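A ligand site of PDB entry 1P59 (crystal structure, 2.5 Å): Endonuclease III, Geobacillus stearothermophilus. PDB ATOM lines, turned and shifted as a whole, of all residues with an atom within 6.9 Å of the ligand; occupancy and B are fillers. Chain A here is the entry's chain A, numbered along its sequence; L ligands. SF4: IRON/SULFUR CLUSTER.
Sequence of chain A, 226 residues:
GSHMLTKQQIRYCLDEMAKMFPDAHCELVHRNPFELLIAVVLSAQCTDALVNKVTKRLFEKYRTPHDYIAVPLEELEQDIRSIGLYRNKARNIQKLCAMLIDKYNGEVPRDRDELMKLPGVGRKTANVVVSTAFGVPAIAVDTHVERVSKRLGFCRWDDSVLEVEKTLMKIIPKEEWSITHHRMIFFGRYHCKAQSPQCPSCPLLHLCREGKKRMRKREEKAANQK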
ATOM      1  N   MET A  17      -8.175 -37.313 -19.206  1.00  0.00           N
ATOM      2  CA  MET A  17      -8.833 -37.638 -20.465  1.00  0.00           C
ATOM      3  C   MET A  17      -9.426 -39.047 -20.386  1.00  0.00           C
ATOM      4  O   MET A  17     -10.403 -39.349 -21.064  1.00  0.00           O
ATOM      5  CB  MET A  17      -7.827 -37.590 -21.618  1.00  0.00           C
ATOM      6  CG  MET A  17      -7.261 -36.232 -21.882  1.00  0.00           C
ATOM      7  SD  MET A  17      -6.031 -36.305 -23.188  1.00  0.00           S
ATOM      8  CE  MET A  17      -5.543 -34.600 -23.309  1.00  0.00           C
ATOM      9  N   VAL A 148      -3.867 -31.496 -29.703  1.00  0.00           N
ATOM     10  CA  VAL A 148      -3.998 -31.657 -28.265  1.00  0.00           C
ATOM     11  C   VAL A 148      -2.631 -31.548 -27.605  1.00  0.00           C
ATOM     12  O   VAL A 148      -2.440 -30.767 -26.680  1.00  0.00           O
ATOM     13  CB  VAL A 148      -4.635 -33.002 -27.905  1.00  0.00           C
ATOM     14  CG1 VAL A 148      -4.507 -33.249 -26.392  1.00  0.00           C
ATOM     15  CG2 VAL A 148      -6.092 -32.996 -28.305  1.00  0.00           C
ATOM     16  N   ARG A 151      -1.359 -27.764 -27.735  1.00  0.00           N
ATOM     17  CA  ARG A 151      -2.067 -26.754 -26.957  1.00  0.00           C
ATOM     18  C   ARG A 151      -1.799 -26.927 -25.460  1.00  0.00           C
ATOM     19  O   ARG A 151      -1.531 -25.946 -24.770  1.00  0.00           O
ATOM     20  CB  ARG A 151      -3.580 -26.853 -27.221  1.00  0.00           C
ATOM     21  CG  ARG A 151      -3.990 -26.270 -28.561  1.00  0.00           C
ATOM     22  CD  ARG A 151      -5.410 -26.668 -28.920  1.00  0.00           C
ATOM     23  NE  ARG A 151      -5.925 -25.880 -30.026  1.00  0.00           N
ATOM     24  CZ  ARG A 151      -7.183 -25.913 -30.436  1.00  0.00           C
ATOM     25  NH1 ARG A 151      -8.066 -26.715 -29.843  1.00  0.00           N
ATOM     26  NH2 ARG A 151      -7.571 -25.142 -31.435  1.00  0.00           N
ATOM     27  N   LEU A 152      -1.861 -28.160 -24.986  1.00  0.00           N
ATOM     28  CA  LEU A 152      -1.634 -28.491 -23.578  1.00  0.00           C
ATOM     29  C   LEU A 152      -0.169 -28.338 -23.165  1.00  0.00           C
ATOM     30  O   LEU A 152       0.150 -28.228 -21.977  1.00  0.00           O
ATOM     31  CB  LEU A 152      -2.085 -29.932 -23.296  1.00  0.00           C
ATOM     32  CG  LEU A 152      -3.193 -30.242 -22.271  1.00  0.00           C
ATOM     33  CD1 LEU A 152      -4.012 -29.018 -21.942  1.00  0.00           C
ATOM     34  CD2 LEU A 152      -4.056 -31.374 -22.841  1.00  0.00           C
ATOM     35  N   PHE A 187     -10.611 -36.772 -26.967  1.00  0.00           N
ATOM     36  CA  PHE A 187     -10.459 -35.517 -26.238  1.00  0.00           C
ATOM     37  C   PHE A 187     -10.395 -34.350 -27.208  1.00  0.00           C
ATOM     38  O   PHE A 187     -10.972 -33.306 -26.965  1.00  0.00           O
ATOM     39  CB  PHE A 187      -9.183 -35.517 -25.399  1.00  0.00           C
ATOM     40  CG  PHE A 187      -8.998 -34.280 -24.591  1.00  0.00           C
ATOM     41  CD1 PHE A 187      -9.700 -34.105 -23.393  1.00  0.00           C
ATOM     42  CD2 PHE A 187      -8.173 -33.259 -25.035  1.00  0.00           C
ATOM     43  CE1 PHE A 187      -9.584 -32.919 -22.671  1.00  0.00           C
ATOM     44  CE2 PHE A 187      -8.045 -32.082 -24.323  1.00  0.00           C
ATOM     45  CZ  PHE A 187      -8.750 -31.903 -23.142  1.00  0.00           C
ATOM     46  N   HIS A 191     -13.815 -32.562 -27.704  1.00  0.00           N
ATOM     47  CA  HIS A 191     -13.721 -31.541 -26.654  1.00  0.00           C
ATOM     48  C   HIS A 191     -12.822 -30.375 -27.049  1.00  0.00           C
ATOM     49  O   HIS A 191     -13.295 -29.253 -27.288  1.00  0.00           O
ATOM     50  CB  HIS A 191     -13.208 -32.170 -25.358  1.00  0.00           C
ATOM     51  CG  HIS A 191     -13.203 -31.221 -24.195  1.00  0.00           C
ATOM     52  ND1 HIS A 191     -14.316 -30.965 -23.439  1.00  0.00           N
ATOM     53  CD2 HIS A 191     -12.218 -30.418 -23.713  1.00  0.00           C
ATOM     54  CE1 HIS A 191     -14.038 -30.044 -22.535  1.00  0.00           C
ATOM     55  NE2 HIS A 191     -12.772 -29.696 -22.683  1.00  0.00           N
ATOM     56  N   CYS A 192     -11.535 -30.649 -27.094  1.00  0.00           N
ATOM     57  CA  CYS A 192     -10.552 -29.650 -27.451  1.00  0.00           C
ATOM     58  C   CYS A 192     -10.549 -29.585 -28.970  1.00  0.00           C
ATOM     59  O   CYS A 192      -9.535 -29.845 -29.620  1.00  0.00           O
ATOM     60  CB  CYS A 192      -9.176 -30.066 -26.923  1.00  0.00           C
ATOM     61  SG  CYS A 192      -7.830 -29.000 -27.431  1.00  0.00           S
ATOM     62  N   LYS A 193     -11.703 -29.241 -29.525  1.00  0.00           N
ATOM     63  CA  LYS A 193     -11.879 -29.163 -30.971  1.00  0.00           C
ATOM     64  C   LYS A 193     -11.117 -27.985 -31.581  1.00  0.00           C
ATOM     65  O   LYS A 193     -11.032 -26.912 -30.983  1.00  0.00           O
ATOM     66  CB  LYS A 193     -13.379 -29.041 -31.314  1.00  0.00           C
ATOM     67  CG  LYS A 193     -14.243 -30.154 -30.723  1.00  0.00           C
ATOM     68  CD  LYS A 193     -15.717 -29.922 -31.025  1.00  0.00           C
ATOM     69  N   PRO A 197     -12.737 -24.920 -29.163  1.00  0.00           N
ATOM     70  CA  PRO A 197     -12.468 -25.777 -27.998  1.00  0.00           C
ATOM     71  C   PRO A 197     -13.347 -25.421 -26.809  1.00  0.00           C
ATOM     72  O   PRO A 197     -13.683 -24.252 -26.605  1.00  0.00           O
ATOM     73  CB  PRO A 197     -10.981 -25.537 -27.735  1.00  0.00           C
ATOM     74  CG  PRO A 197     -10.792 -24.125 -28.194  1.00  0.00           C
ATOM     75  CD  PRO A 197     -11.551 -24.113 -29.495  1.00  0.00           C
ATOM     76  N   GLN A 198     -13.708 -26.427 -26.006  1.00  0.00           N
ATOM     77  CA  GLN A 198     -14.544 -26.232 -24.829  1.00  0.00           C
ATOM     78  C   GLN A 198     -13.697 -25.886 -23.607  1.00  0.00           C
ATOM     79  O   GLN A 198     -13.834 -26.497 -22.544  1.00  0.00           O
ATOM     80  CB  GLN A 198     -15.381 -27.498 -24.570  1.00  0.00           C
ATOM     81  N   CYS A 199     -12.816 -24.900 -23.775  1.00  0.00           N
ATOM     82  CA  CYS A 199     -11.910 -24.458 -22.710  1.00  0.00           C
ATOM     83  C   CYS A 199     -12.630 -24.073 -21.411  1.00  0.00           C
ATOM     84  O   CYS A 199     -12.233 -24.504 -20.333  1.00  0.00           O
ATOM     85  CB  CYS A 199     -11.066 -23.274 -23.191  1.00  0.00           C
ATOM     86  SG  CYS A 199     -10.323 -23.478 -24.820  1.00  0.00           S
ATOM     87  N   PRO A 200     -13.681 -23.239 -21.503  1.00  0.00           N
ATOM     88  CA  PRO A 200     -14.465 -22.775 -20.349  1.00  0.00           C
ATOM     89  C   PRO A 200     -14.768 -23.851 -19.308  1.00  0.00           C
ATOM     90  O   PRO A 200     -14.759 -23.579 -18.097  1.00  0.00           O
ATOM     91  CB  PRO A 200     -15.735 -22.230 -20.994  1.00  0.00           C
ATOM     92  CG  PRO A 200     -15.215 -21.625 -22.258  1.00  0.00           C
ATOM     93  CD  PRO A 200     -14.243 -22.690 -22.762  1.00  0.00           C
ATOM     94  N   SER A 201     -15.050 -25.059 -19.769  1.00  0.00           N
ATOM     95  CA  SER A 201     -15.378 -26.170 -18.886  1.00  0.00           C
ATOM     96  C   SER A 201     -14.314 -27.261 -18.934  1.00  0.00           C
ATOM     97  O   SER A 201     -14.571 -28.411 -18.539  1.00  0.00           O
ATOM     98  CB  SER A 201     -16.724 -26.768 -19.302  1.00  0.00           C
ATOM     99  OG  SER A 201     -16.645 -27.371 -20.588  1.00  0.00           O
ATOM    100  N   CYS A 202     -13.128 -26.928 -19.417  1.00  0.00           N
ATOM    101  CA  CYS A 202     -12.086 -27.938 -19.522  1.00  0.00           C
ATOM    102  C   CYS A 202     -11.352 -28.178 -18.220  1.00  0.00           C
ATOM    103  O   CYS A 202     -10.708 -27.280 -17.667  1.00  0.00           O
ATOM    104  CB  CYS A 202     -11.084 -27.576 -20.610  1.00  0.00           C
ATOM    105  SG  CYS A 202      -9.863 -28.880 -20.784  1.00  0.00           S
ATOM    106  N   PRO A 203     -11.423 -29.423 -17.717  1.00  0.00           N
ATOM    107  CA  PRO A 203     -10.793 -29.890 -16.474  1.00  0.00           C
ATOM    108  C   PRO A 203      -9.284 -29.681 -16.476  1.00  0.00           C
ATOM    109  O   PRO A 203      -8.611 -29.906 -15.470  1.00  0.00           O
ATOM    110  CB  PRO A 203     -11.135 -31.382 -16.450  1.00  0.00           C
ATOM    111  CG  PRO A 203     -12.378 -31.484 -17.299  1.00  0.00           C
ATOM    112  CD  PRO A 203     -12.074 -30.537 -18.415  1.00  0.00           C
ATOM    113  N   LEU A 204      -8.758 -29.251 -17.625  1.00  0.00           N
ATOM    114  CA  LEU A 204      -7.329 -29.029 -17.787  1.00  0.00           C
ATOM    115  C   LEU A 204      -6.961 -27.572 -18.030  1.00  0.00           C
ATOM    116  O   LEU A 204      -5.791 -27.231 -18.243  1.00  0.00           O
ATOM    117  CB  LEU A 204      -6.807 -29.897 -18.936  1.00  0.00           C
ATOM    118  CG  LEU A 204      -6.908 -31.414 -18.716  1.00  0.00           C
ATOM    119  CD1 LEU A 204      -6.428 -32.143 -19.960  1.00  0.00           C
ATOM    120  CD2 LEU A 204      -6.085 -31.818 -17.510  1.00  0.00           C
ATOM    121  N   LEU A 205      -7.959 -26.703 -18.000  1.00  0.00           N
ATOM    122  CA  LEU A 205      -7.711 -25.284 -18.211  1.00  0.00           C
ATOM    123  C   LEU A 205      -6.666 -24.757 -17.201  1.00  0.00           C
ATOM    124  O   LEU A 205      -5.865 -23.889 -17.545  1.00  0.00           O
ATOM    125  CB  LEU A 205      -9.006 -24.485 -18.063  1.00  0.00           C
ATOM    126  CG  LEU A 205      -9.221 -23.325 -19.040  1.00  0.00           C
ATOM    127  CD1 LEU A 205     -10.266 -22.404 -18.428  1.00  0.00           C
ATOM    128  CD2 LEU A 205      -7.944 -22.570 -19.306  1.00  0.00           C
ATOM    129  N   HIS A 206      -6.680 -25.290 -15.980  1.00  0.00           N
ATOM    130  CA  HIS A 206      -5.764 -24.811 -14.940  1.00  0.00           C
ATOM    131  C   HIS A 206      -4.276 -24.921 -15.267  1.00  0.00           C
ATOM    132  O   HIS A 206      -3.477 -24.114 -14.772  1.00  0.00           O
ATOM    133  CB  HIS A 206      -6.028 -25.483 -13.590  1.00  0.00           C
ATOM    134  CG  HIS A 206      -5.727 -26.943 -13.538  1.00  0.00           C
ATOM    135  ND1 HIS A 206      -6.672 -27.906 -13.833  1.00  0.00           N
ATOM    136  CD2 HIS A 206      -4.577 -27.612 -13.265  1.00  0.00           C
ATOM    137  CE1 HIS A 206      -6.120 -29.104 -13.729  1.00  0.00           C
ATOM    138  NE2 HIS A 206      -4.849 -28.956 -13.395  1.00  0.00           N
ATOM    139  N   CYS A 208      -3.360 -25.503 -18.663  1.00  0.00           N
ATOM    140  CA  CYS A 208      -3.288 -25.352 -20.101  1.00  0.00           C
ATOM    141  C   CYS A 208      -3.073 -23.932 -20.576  1.00  0.00           C
ATOM    142  O   CYS A 208      -3.997 -23.126 -20.551  1.00  0.00           O
ATOM    143  CB  CYS A 208      -4.558 -25.898 -20.763  1.00  0.00           C
ATOM    144  SG  CYS A 208      -4.532 -25.697 -22.567  1.00  0.00           S
ATOM    145  N   ARG A 209      -1.854 -23.642 -21.027  1.00  0.00           N
ATOM    146  CA  ARG A 209      -1.516 -22.310 -21.512  1.00  0.00           C
ATOM    147  C   ARG A 209      -2.460 -21.858 -22.628  1.00  0.00           C
ATOM    148  O   ARG A 209      -2.823 -20.684 -22.694  1.00  0.00           O
ATOM    149  CB  ARG A 209      -0.075 -22.283 -22.018  1.00  0.00           C
ATOM    150  N   GLU A 210      -2.844 -22.791 -23.487  1.00  0.00           N
ATOM    151  CA  GLU A 210      -3.734 -22.482 -24.608  1.00  0.00           C
ATOM    152  C   GLU A 210      -5.127 -22.115 -24.147  1.00  0.00           C
ATOM    153  O   GLU A 210      -5.768 -21.258 -24.734  1.00  0.00           O
ATOM    154  CB  GLU A 210      -3.848 -23.675 -25.567  1.00  0.00           C
ATOM    155  CG  GLU A 210      -4.638 -23.345 -26.827  1.00  0.00           C
ATOM    156  CD  GLU A 210      -3.970 -22.255 -27.650  1.00  0.00           C
ATOM    157  OE1 GLU A 210      -4.584 -21.769 -28.615  1.00  0.00           O
ATOM    158  OE2 GLU A 210      -2.824 -21.893 -27.329  1.00  0.00           O
ATOM    159  N   GLY A 211      -5.595 -22.792 -23.102  1.00  0.00           N
ATOM    160  CA  GLY A 211      -6.903 -22.498 -22.566  1.00  0.00           C
ATOM    161  C   GLY A 211      -6.912 -21.084 -21.987  1.00  0.00           C
ATOM    162  O   GLY A 211      -7.681 -20.229 -22.432  1.00  0.00           O
ATOM    163  N   LYS A 212      -6.043 -20.848 -21.009  1.00  0.00           N
ATOM    164  CA  LYS A 212      -5.943 -19.534 -20.365  1.00  0.00           C
ATOM    165  C   LYS A 212      -5.868 -18.449 -21.445  1.00  0.00           C
ATOM    166  O   LYS A 212      -6.632 -17.479 -21.415  1.00  0.00           O
ATOM    167  CB  LYS A 212      -4.699 -19.460 -19.473  1.00  0.00           C
ATOM    168  CG  LYS A 212      -4.632 -20.492 -18.360  1.00  0.00           C
ATOM    169  CD  LYS A 212      -3.280 -20.418 -17.661  1.00  0.00           C
ATOM    170  CE  LYS A 212      -3.037 -21.563 -16.664  1.00  0.00           C
ATOM    171  NZ  LYS A 212      -3.812 -21.443 -15.389  1.00  0.00           N
ATOM    172  N   ARG A 214      -6.821 -18.491 -24.474  1.00  0.00           N
ATOM    173  CA  ARG A 214      -8.114 -18.364 -25.145  1.00  0.00           C
ATOM    174  C   ARG A 214      -9.167 -17.693 -24.269  1.00  0.00           C
ATOM    175  O   ARG A 214     -10.032 -16.967 -24.774  1.00  0.00           O
ATOM    176  CB  ARG A 214      -8.626 -19.737 -25.602  1.00  0.00           C
ATOM    177  CG  ARG A 214      -8.114 -20.170 -26.961  1.00  0.00           C
ATOM    178  CD  ARG A 214      -8.534 -21.598 -27.291  1.00  0.00           C
ATOM    179  NE  ARG A 214      -8.111 -22.002 -28.637  1.00  0.00           N
ATOM    180  CZ  ARG A 214      -8.767 -21.679 -29.758  1.00  0.00           C
ATOM    181  NH1 ARG A 214      -9.883 -20.962 -29.685  1.00  0.00           N
ATOM    182  NH2 ARG A 214      -8.294 -22.057 -30.929  1.00  0.00           N
ATOM    183  N   MET A 215      -9.110 -17.940 -22.964  1.00  0.00           N
ATOM    184  CA  MET A 215     -10.059 -17.357 -22.020  1.00  0.00           C
ATOM    185  C   MET A 215      -9.937 -15.848 -21.993  1.00  0.00           C
ATOM    186  O   MET A 215     -10.940 -15.130 -22.028  1.00  0.00           O
ATOM    187  CB  MET A 215      -9.842 -17.916 -20.615  1.00  0.00           C
ATOM    188  CG  MET A 215     -10.090 -19.410 -20.503  1.00  0.00           C
ATOM    189  SD  MET A 215     -11.765 -19.872 -20.962  1.00  0.00           S
ATOM    190  CE  MET A 215     -12.539 -19.978 -19.336  1.00  0.00           C
HETATM  191 FE1  SF4 L   1      -8.962 -27.611 -22.533  1.00  0.00          FE
HETATM  192 FE2  SF4 L   1      -8.086 -27.621 -25.201  1.00  0.00          FE
HETATM  193 FE3  SF4 L   1      -9.106 -25.475 -24.049  1.00  0.00          FE
HETATM  194 FE4  SF4 L   1      -6.663 -26.431 -23.452  1.00  0.00          FE
HETATM  195  S1  SF4 L   1      -7.367 -25.553 -25.480  1.00  0.00           S
HETATM  196  S2  SF4 L   1      -8.145 -25.651 -22.175  1.00  0.00           S
HETATM  197  S3  SF4 L   1      -7.093 -28.681 -23.586  1.00  0.00           S
HETATM  198  S4  SF4 L   1     -10.225 -27.230 -24.329  1.00  0.00           S
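Merely in contact with the ligand: Leu 152 (3.5 Å), Phe 187 (3.6 Å), His 191 (3.8 Å), Pro 197 (3.9 Å), Gln 198 (3.8 Å), Glu 210 (3.8 Å) and Gly 211 (3.4 Å). Hydrophobic or aromatic side chains within 4 Å of the ligand: Leu 152, Phe 187, His 191 and Pro 197. Of the 25 residues printed, 11 come within 4 Å of the ligand. The nearest printed residue that does not touch the ligand is Leu 205 (4.005 Å).
An iron atom (FE1) of the ligand is bound by the side-chain sulfur of Cys 202 (2.3 Å). SG of Cys 208 binds FE4 of the ligand (2.4 Å). S4 of the ligand lies close to N of Cys 199 (3.5 Å). FE3 of the ligand is bound by SG of Cys 199. An iron atom (FE2) of the ligand is bound by the side-chain sulfur (SG) of Cys 192.
A ring nitrogen (NE2) of His 191 lies close to the side-chain sulfur (SG) of Cys 202, at 3.6 Å. SG of Cys 208 sits close to N of Gly 211, 3.1 Å away. The backbone NH (N) of Glu 210 lies close to the side-chain sulfur (SG) of Cys 208. SG of Cys 208 sits close to O of Arg 151 (3.7 Å). The backbone NH (N) of Cys 192 is in hydrogen-bond range of the backbone carbonyl oxygen (O) of Phe 187 (2.7 Å). NH1 of Arg 151 lies within hydrogen-bond range of O of Cys 192, 3.5 Å away. The side-chain carboxylate of Glu 210 is in salt-bridge range of the guanidinium group of Arg 214. The backbone carbonyl oxygen of His 191 sits at hydrogen-bond distance from the backbone NH of Gln 198 (3.1 Å).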
